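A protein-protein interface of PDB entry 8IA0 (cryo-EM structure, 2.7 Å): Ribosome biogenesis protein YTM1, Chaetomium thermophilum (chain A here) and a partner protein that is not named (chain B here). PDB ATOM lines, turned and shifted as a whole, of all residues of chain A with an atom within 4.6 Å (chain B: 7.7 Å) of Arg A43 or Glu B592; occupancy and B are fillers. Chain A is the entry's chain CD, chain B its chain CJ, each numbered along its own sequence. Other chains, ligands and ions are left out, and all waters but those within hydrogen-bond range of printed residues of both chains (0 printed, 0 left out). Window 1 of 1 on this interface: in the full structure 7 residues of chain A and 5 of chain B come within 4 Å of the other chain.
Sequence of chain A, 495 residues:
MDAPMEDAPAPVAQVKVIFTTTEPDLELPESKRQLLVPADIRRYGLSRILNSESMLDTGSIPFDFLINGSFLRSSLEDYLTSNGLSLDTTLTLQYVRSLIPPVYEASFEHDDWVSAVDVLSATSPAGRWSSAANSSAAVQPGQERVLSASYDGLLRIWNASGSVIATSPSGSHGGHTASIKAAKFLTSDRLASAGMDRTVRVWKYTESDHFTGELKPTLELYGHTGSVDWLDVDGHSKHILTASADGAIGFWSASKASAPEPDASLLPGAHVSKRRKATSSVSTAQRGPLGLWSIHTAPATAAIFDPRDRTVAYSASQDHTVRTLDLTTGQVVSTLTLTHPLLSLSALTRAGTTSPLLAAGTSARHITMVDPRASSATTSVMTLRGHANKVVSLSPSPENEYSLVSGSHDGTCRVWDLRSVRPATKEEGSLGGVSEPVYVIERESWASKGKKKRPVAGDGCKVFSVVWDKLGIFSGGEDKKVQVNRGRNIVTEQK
The side-chain carboxylate (OE2) of Glu B592 lies within salt-bridge range of the guanidinium group (NE) of Arg A43, at 3.6 Å.
The side-chain carboxylate (OE2) of Glu B592 is in hydrogen-bond range of the backbone NH (N) of Tyr A44 (2.6 Å).
The side-chain amide oxygen (OE1) of Gln B588 lies close to the side-chain carboxylate (OE1) of Glu B592.
NH1 of Arg B589 lies within salt-bridge range of OE1 of Glu B592 (2.6 Å).
Among the printed residues, merely in contact across the chains: Arg A42 with Glu B592 (3.3 Å).
Of the printed residues of chain B, Arg A42 touches Glu B592 (3.3 Å).
Arg A43 touches one residue of chain B.
Printed residues of chain B within 4 Å of Tyr A44: Glu B592.
Asp A64 touches none of the printed residues of chain B.
Arg B589 touches none of the printed residues of chain A.
Glu B592 touches just these residues of chain A: Arg A42, Arg A43 and Tyr A44.
The nearest printed residue of chain A that does not touch Glu B592 is Gly A45 (5.2 Å).
The nearest printed residue of chain B that does not touch Arg A42 is Gln B588 (4.5 Å).
Of the 10 printed residues of chain A, 3 touch a printed residue of chain B.
Printed residues of chain A that touch a printed residue of chain B: Arg A42, Arg A43 and Tyr A44.
Hydrophobic or aromatic side chains of chain A within 4 Å of the printed part of chain B: Tyr A44.
Printed residues of chain B that touch a printed residue of chain A: Glu B592.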
ATOM      1  N   ILE A  41      25.697 -13.916 -17.307  1.00  0.00           N
ATOM      2  CA  ILE A  41      24.403 -14.110 -17.946  1.00  0.00           C
ATOM      3  C   ILE A  41      23.838 -15.483 -17.590  1.00  0.00           C
ATOM      4  O   ILE A  41      24.567 -16.442 -17.316  1.00  0.00           O
ATOM      5  CB  ILE A  41      24.520 -13.920 -19.470  1.00  0.00           C
ATOM      6  CG1 ILE A  41      23.140 -13.748 -20.111  1.00  0.00           C
ATOM      7  CG2 ILE A  41      25.286 -15.074 -20.094  1.00  0.00           C
ATOM      8  CD1 ILE A  41      23.190 -13.257 -21.541  1.00  0.00           C
ATOM      9  N   ARG A  42      22.512 -15.570 -17.589  1.00  0.00           N
ATOM     10  CA  ARG A  42      21.771 -16.788 -17.297  1.00  0.00           C
ATOM     11  C   ARG A  42      21.445 -17.527 -18.591  1.00  0.00           C
ATOM     12  O   ARG A  42      21.320 -16.924 -19.660  1.00  0.00           O
ATOM     13  CB  ARG A  42      20.483 -16.453 -16.536  1.00  0.00           C
ATOM     14  CG  ARG A  42      19.689 -17.643 -16.013  1.00  0.00           C
ATOM     15  CD  ARG A  42      20.554 -18.619 -15.234  1.00  0.00           C
ATOM     16  NE  ARG A  42      21.326 -17.960 -14.189  1.00  0.00           N
ATOM     17  CZ  ARG A  42      22.394 -18.488 -13.608  1.00  0.00           C
ATOM     18  NH1 ARG A  42      22.819 -19.701 -13.917  1.00  0.00           N
ATOM     19  NH2 ARG A  42      23.048 -17.783 -12.688  1.00  0.00           N
ATOM     20  N   ARG A  43      21.300 -18.853 -18.480  1.00  0.00           N
ATOM     21  CA  ARG A  43      21.019 -19.685 -19.647  1.00  0.00           C
ATOM     22  C   ARG A  43      19.764 -19.241 -20.386  1.00  0.00           C
ATOM     23  O   ARG A  43      19.676 -19.434 -21.603  1.00  0.00           O
ATOM     24  CB  ARG A  43      20.885 -21.152 -19.234  1.00  0.00           C
ATOM     25  CG  ARG A  43      20.861 -22.126 -20.403  1.00  0.00           C
ATOM     26  CD  ARG A  43      19.726 -23.133 -20.274  1.00  0.00           C
ATOM     27  NE  ARG A  43      18.420 -22.500 -20.129  1.00  0.00           N
ATOM     28  CZ  ARG A  43      17.806 -21.805 -21.077  1.00  0.00           C
ATOM     29  NH1 ARG A  43      18.341 -21.649 -22.278  1.00  0.00           N
ATOM     30  NH2 ARG A  43      16.621 -21.261 -20.819  1.00  0.00           N
ATOM     31  N   TYR A  44      18.798 -18.651 -19.681  1.00  0.00           N
ATOM     32  CA  TYR A  44      17.660 -18.034 -20.354  1.00  0.00           C
ATOM     33  C   TYR A  44      18.126 -16.925 -21.287  1.00  0.00           C
ATOM     34  O   TYR A  44      17.598 -16.763 -22.393  1.00  0.00           O
ATOM     35  CB  TYR A  44      16.676 -17.497 -19.313  1.00  0.00           C
ATOM     36  CG  TYR A  44      15.593 -16.595 -19.865  1.00  0.00           C
ATOM     37  CD1 TYR A  44      14.492 -17.124 -20.527  1.00  0.00           C
ATOM     38  CD2 TYR A  44      15.665 -15.216 -19.710  1.00  0.00           C
ATOM     39  CE1 TYR A  44      13.497 -16.303 -21.025  1.00  0.00           C
ATOM     40  CE2 TYR A  44      14.676 -14.388 -20.207  1.00  0.00           C
ATOM     41  CZ  TYR A  44      13.595 -14.936 -20.864  1.00  0.00           C
ATOM     42  OH  TYR A  44      12.608 -14.116 -21.359  1.00  0.00           O
ATOM     43  N   GLY A  45      19.130 -16.156 -20.857  1.00  0.00           N
ATOM     44  CA  GLY A  45      19.654 -15.090 -21.691  1.00  0.00           C
ATOM     45  C   GLY A  45      20.300 -15.581 -22.971  1.00  0.00           C
ATOM     46  O   GLY A  45      20.067 -15.011 -24.041  1.00  0.00           O
ATOM     47  N   LEU A  46      21.120 -16.634 -22.886  1.00  0.00           N
ATOM     48  CA  LEU A  46      21.705 -17.194 -24.101  1.00  0.00           C
ATOM     49  C   LEU A  46      20.633 -17.740 -25.032  1.00  0.00           C
ATOM     50  O   LEU A  46      20.803 -17.734 -26.256  1.00  0.00           O
ATOM     51  CB  LEU A  46      22.734 -18.279 -23.773  1.00  0.00           C
ATOM     52  CG  LEU A  46      23.939 -17.959 -22.884  1.00  0.00           C
ATOM     53  CD1 LEU A  46      24.515 -16.597 -23.245  1.00  0.00           C
ATOM     54  CD2 LEU A  46      23.632 -18.051 -21.402  1.00  0.00           C
ATOM     55  N   SER A  47      19.523 -18.224 -24.474  1.00  0.00           N
ATOM     56  CA  SER A  47      18.407 -18.636 -25.318  1.00  0.00           C
ATOM     57  C   SER A  47      17.830 -17.451 -26.081  1.00  0.00           C
ATOM     58  O   SER A  47      17.539 -17.556 -27.278  1.00  0.00           O
ATOM     59  CB  SER A  47      17.326 -19.309 -24.473  1.00  0.00           C
ATOM     60  OG  SER A  47      16.211 -19.671 -25.269  1.00  0.00           O
ATOM     61  N   PHE A  63      17.408 -23.964 -26.848  1.00  0.00           N
ATOM     62  CA  PHE A  63      18.666 -24.631 -27.136  1.00  0.00           C
ATOM     63  C   PHE A  63      19.411 -24.919 -25.841  1.00  0.00           C
ATOM     64  O   PHE A  63      19.262 -24.205 -24.845  1.00  0.00           O
ATOM     65  CB  PHE A  63      19.559 -23.793 -28.061  1.00  0.00           C
ATOM     66  CG  PHE A  63      19.057 -23.700 -29.473  1.00  0.00           C
ATOM     67  CD1 PHE A  63      18.191 -22.688 -29.850  1.00  0.00           C
ATOM     68  CD2 PHE A  63      19.459 -24.622 -30.425  1.00  0.00           C
ATOM     69  CE1 PHE A  63      17.733 -22.599 -31.150  1.00  0.00           C
ATOM     70  CE2 PHE A  63      19.004 -24.538 -31.726  1.00  0.00           C
ATOM     71  CZ  PHE A  63      18.139 -23.525 -32.089  1.00  0.00           C
ATOM     72  N   ASP A  64      20.210 -25.981 -25.865  1.00  0.00           N
ATOM     73  CA  ASP A  64      21.090 -26.338 -24.764  1.00  0.00           C
ATOM     74  C   ASP A  64      22.536 -26.300 -25.237  1.00  0.00           C
ATOM     75  O   ASP A  64      22.860 -26.770 -26.332  1.00  0.00           O
ATOM     76  CB  ASP A  64      20.758 -27.727 -24.206  1.00  0.00           C
ATOM     77  CG  ASP A  64      19.524 -27.722 -23.325  1.00  0.00           C
ATOM     78  OD1 ASP A  64      19.249 -26.682 -22.691  1.00  0.00           O
ATOM     79  OD2 ASP A  64      18.828 -28.758 -23.268  1.00  0.00           O
ATOM     80  N   LEU A  72      26.140 -26.375 -19.709  1.00  0.00           N
ATOM     81  CA  LEU A  72      26.252 -25.139 -18.938  1.00  0.00           C
ATOM     82  C   LEU A  72      25.074 -25.077 -17.978  1.00  0.00           C
ATOM     83  O   LEU A  72      23.983 -24.629 -18.339  1.00  0.00           O
ATOM     84  CB  LEU A  72      26.277 -23.929 -19.865  1.00  0.00           C
ATOM     85  CG  LEU A  72      26.546 -22.569 -19.220  1.00  0.00           C
ATOM     86  CD1 LEU A  72      27.978 -22.485 -18.707  1.00  0.00           C
ATOM     87  CD2 LEU A  72      26.256 -21.446 -20.205  1.00  0.00           C
ATOM     88  N   LEU B 585      17.235 -25.018  -8.183  1.00  0.00           N
ATOM     89  CA  LEU B 585      17.810 -25.415  -9.465  1.00  0.00           C
ATOM     90  C   LEU B 585      16.741 -25.945 -10.413  1.00  0.00           C
ATOM     91  O   LEU B 585      16.720 -25.601 -11.601  1.00  0.00           O
ATOM     92  CB  LEU B 585      18.899 -26.466  -9.241  1.00  0.00           C
ATOM     93  CG  LEU B 585      19.574 -27.050 -10.484  1.00  0.00           C
ATOM     94  CD1 LEU B 585      20.489 -26.021 -11.127  1.00  0.00           C
ATOM     95  CD2 LEU B 585      20.342 -28.316 -10.137  1.00  0.00           C
ATOM     96  N   GLU B 586      15.845 -26.792  -9.905  1.00  0.00           N
ATOM     97  CA  GLU B 586      14.776 -27.327 -10.741  1.00  0.00           C
ATOM     98  C   GLU B 586      13.755 -26.250 -11.085  1.00  0.00           C
ATOM     99  O   GLU B 586      13.221 -26.218 -12.200  1.00  0.00           O
ATOM    100  CB  GLU B 586      14.099 -28.503 -10.036  1.00  0.00           C
ATOM    101  CG  GLU B 586      14.986 -29.725  -9.867  1.00  0.00           C
ATOM    102  CD  GLU B 586      15.330 -30.381 -11.189  1.00  0.00           C
ATOM    103  OE1 GLU B 586      14.476 -30.367 -12.101  1.00  0.00           O
ATOM    104  OE2 GLU B 586      16.452 -30.913 -11.316  1.00  0.00           O
ATOM    105  N   ARG B 587      13.463 -25.362 -10.130  1.00  0.00           N
ATOM    106  CA  ARG B 587      12.399 -24.381 -10.326  1.00  0.00           C
ATOM    107  C   ARG B 587      12.698 -23.448 -11.490  1.00  0.00           C
ATOM    108  O   ARG B 587      11.831 -23.202 -12.336  1.00  0.00           O
ATOM    109  CB  ARG B 587      12.185 -23.570  -9.048  1.00  0.00           C
ATOM    110  CG  ARG B 587      11.261 -22.375  -9.234  1.00  0.00           C
ATOM    111  CD  ARG B 587      10.733 -21.857  -7.907  1.00  0.00           C
ATOM    112  NE  ARG B 587      11.404 -20.629  -7.499  1.00  0.00           N
ATOM    113  CZ  ARG B 587      12.069 -20.478  -6.362  1.00  0.00           C
ATOM    114  NH1 ARG B 587      12.173 -21.465  -5.487  1.00  0.00           N
ATOM    115  NH2 ARG B 587      12.646 -19.310  -6.096  1.00  0.00           N
ATOM    116  N   GLN B 588      13.922 -22.918 -11.556  1.00  0.00           N
ATOM    117  CA  GLN B 588      14.228 -21.973 -12.624  1.00  0.00           C
ATOM    118  C   GLN B 588      14.421 -22.677 -13.960  1.00  0.00           C
ATOM    119  O   GLN B 588      14.350 -22.029 -15.010  1.00  0.00           O
ATOM    120  CB  GLN B 588      15.446 -21.120 -12.257  1.00  0.00           C
ATOM    121  CG  GLN B 588      16.592 -21.847 -11.581  1.00  0.00           C
ATOM    122  CD  GLN B 588      17.648 -22.326 -12.545  1.00  0.00           C
ATOM    123  OE1 GLN B 588      17.760 -21.830 -13.666  1.00  0.00           O
ATOM    124  NE2 GLN B 588      18.449 -23.287 -12.104  1.00  0.00           N
ATOM    125  N   ARG B 589      14.649 -23.991 -13.951  1.00  0.00           N
ATOM    126  CA  ARG B 589      14.601 -24.750 -15.197  1.00  0.00           C
ATOM    127  C   ARG B 589      13.190 -24.774 -15.768  1.00  0.00           C
ATOM    128  O   ARG B 589      12.996 -24.623 -16.979  1.00  0.00           O
ATOM    129  CB  ARG B 589      15.115 -26.171 -14.977  1.00  0.00           C
ATOM    130  CG  ARG B 589      15.650 -26.824 -16.243  1.00  0.00           C
ATOM    131  CD  ARG B 589      17.004 -26.312 -16.744  1.00  0.00           C
ATOM    132  NE  ARG B 589      18.036 -26.204 -15.716  1.00  0.00           N
ATOM    133  CZ  ARG B 589      18.302 -25.121 -15.000  1.00  0.00           C
ATOM    134  NH1 ARG B 589      17.666 -23.980 -15.204  1.00  0.00           N
ATOM    135  NH2 ARG B 589      19.257 -25.177 -14.077  1.00  0.00           N
ATOM    136  N   GLU B 590      12.188 -24.960 -14.905  1.00  0.00           N
ATOM    137  CA  GLU B 590      10.806 -24.989 -15.373  1.00  0.00           C
ATOM    138  C   GLU B 590      10.390 -23.651 -15.965  1.00  0.00           C
ATOM    139  O   GLU B 590       9.729 -23.610 -17.008  1.00  0.00           O
ATOM    140  CB  GLU B 590       9.861 -25.386 -14.235  1.00  0.00           C
ATOM    141  CG  GLU B 590      10.231 -26.606 -13.350  1.00  0.00           C
ATOM    142  CD  GLU B 590      10.882 -27.816 -14.048  1.00  0.00           C
ATOM    143  OE1 GLU B 590      11.147 -28.803 -13.327  1.00  0.00           O
ATOM    144  OE2 GLU B 590      11.095 -27.834 -15.281  1.00  0.00           O
ATOM    145  N   LEU B 591      10.756 -22.545 -15.316  1.00  0.00           N
ATOM    146  CA  LEU B 591      10.414 -21.243 -15.872  1.00  0.00           C
ATOM    147  C   LEU B 591      11.305 -20.871 -17.049  1.00  0.00           C
ATOM    148  O   LEU B 591      10.861 -20.131 -17.933  1.00  0.00           O
ATOM    149  CB  LEU B 591      10.472 -20.162 -14.787  1.00  0.00           C
ATOM    150  CG  LEU B 591      11.796 -19.806 -14.115  1.00  0.00           C
ATOM    151  CD1 LEU B 591      12.440 -18.607 -14.792  1.00  0.00           C
ATOM    152  CD2 LEU B 591      11.566 -19.525 -12.639  1.00  0.00           C
ATOM    153  N   GLU B 592      12.546 -21.362 -17.086  1.00  0.00           N
ATOM    154  CA  GLU B 592      13.355 -21.189 -18.286  1.00  0.00           C
ATOM    155  C   GLU B 592      12.828 -22.030 -19.437  1.00  0.00           C
ATOM    156  O   GLU B 592      12.952 -21.630 -20.600  1.00  0.00           O
ATOM    157  CB  GLU B 592      14.817 -21.542 -18.008  1.00  0.00           C
ATOM    158  CG  GLU B 592      15.627 -20.402 -17.412  1.00  0.00           C
ATOM    159  CD  GLU B 592      17.080 -20.775 -17.191  1.00  0.00           C
ATOM    160  OE1 GLU B 592      17.337 -21.841 -16.595  1.00  0.00           O
ATOM    161  OE2 GLU B 592      17.967 -19.999 -17.608  1.00  0.00           O
ATOM    162  N   ALA B 593      12.246 -23.193 -19.133  1.00  0.00           N
ATOM    163  CA  ALA B 593      11.596 -23.987 -20.169  1.00  0.00           C
ATOM    164  C   ALA B 593      10.423 -23.232 -20.779  1.00  0.00           C
ATOM    165  O   ALA B 593      10.221 -23.261 -21.999  1.00  0.00           O
ATOM    166  CB  ALA B 593      11.135 -25.325 -19.595  1.00  0.00           C
ATOM    167  N   GLU B 594       9.643 -22.549 -19.949  1.00  0.00           N
ATOM    168  CA  GLU B 594       8.541 -21.733 -20.437  1.00  0.00           C
ATOM    169  C   GLU B 594       8.864 -20.253 -20.274  1.00  0.00           C
ATOM    170  O   GLU B 594       9.827 -19.751 -20.852  1.00  0.00           O
ATOM    171  CB  GLU B 594       7.242 -22.082 -19.703  1.00  0.00           C
ATOM    172  CG  GLU B 594       6.025 -21.167 -19.964  1.00  0.00           C
ATOM    173  CD  GLU B 594       5.871 -20.655 -21.399  1.00  0.00           C
ATOM    174  OE1 GLU B 594       5.148 -19.652 -21.578  1.00  0.00           O
ATOM    175  OE2 GLU B 594       6.393 -21.270 -22.355  1.00  0.00           O
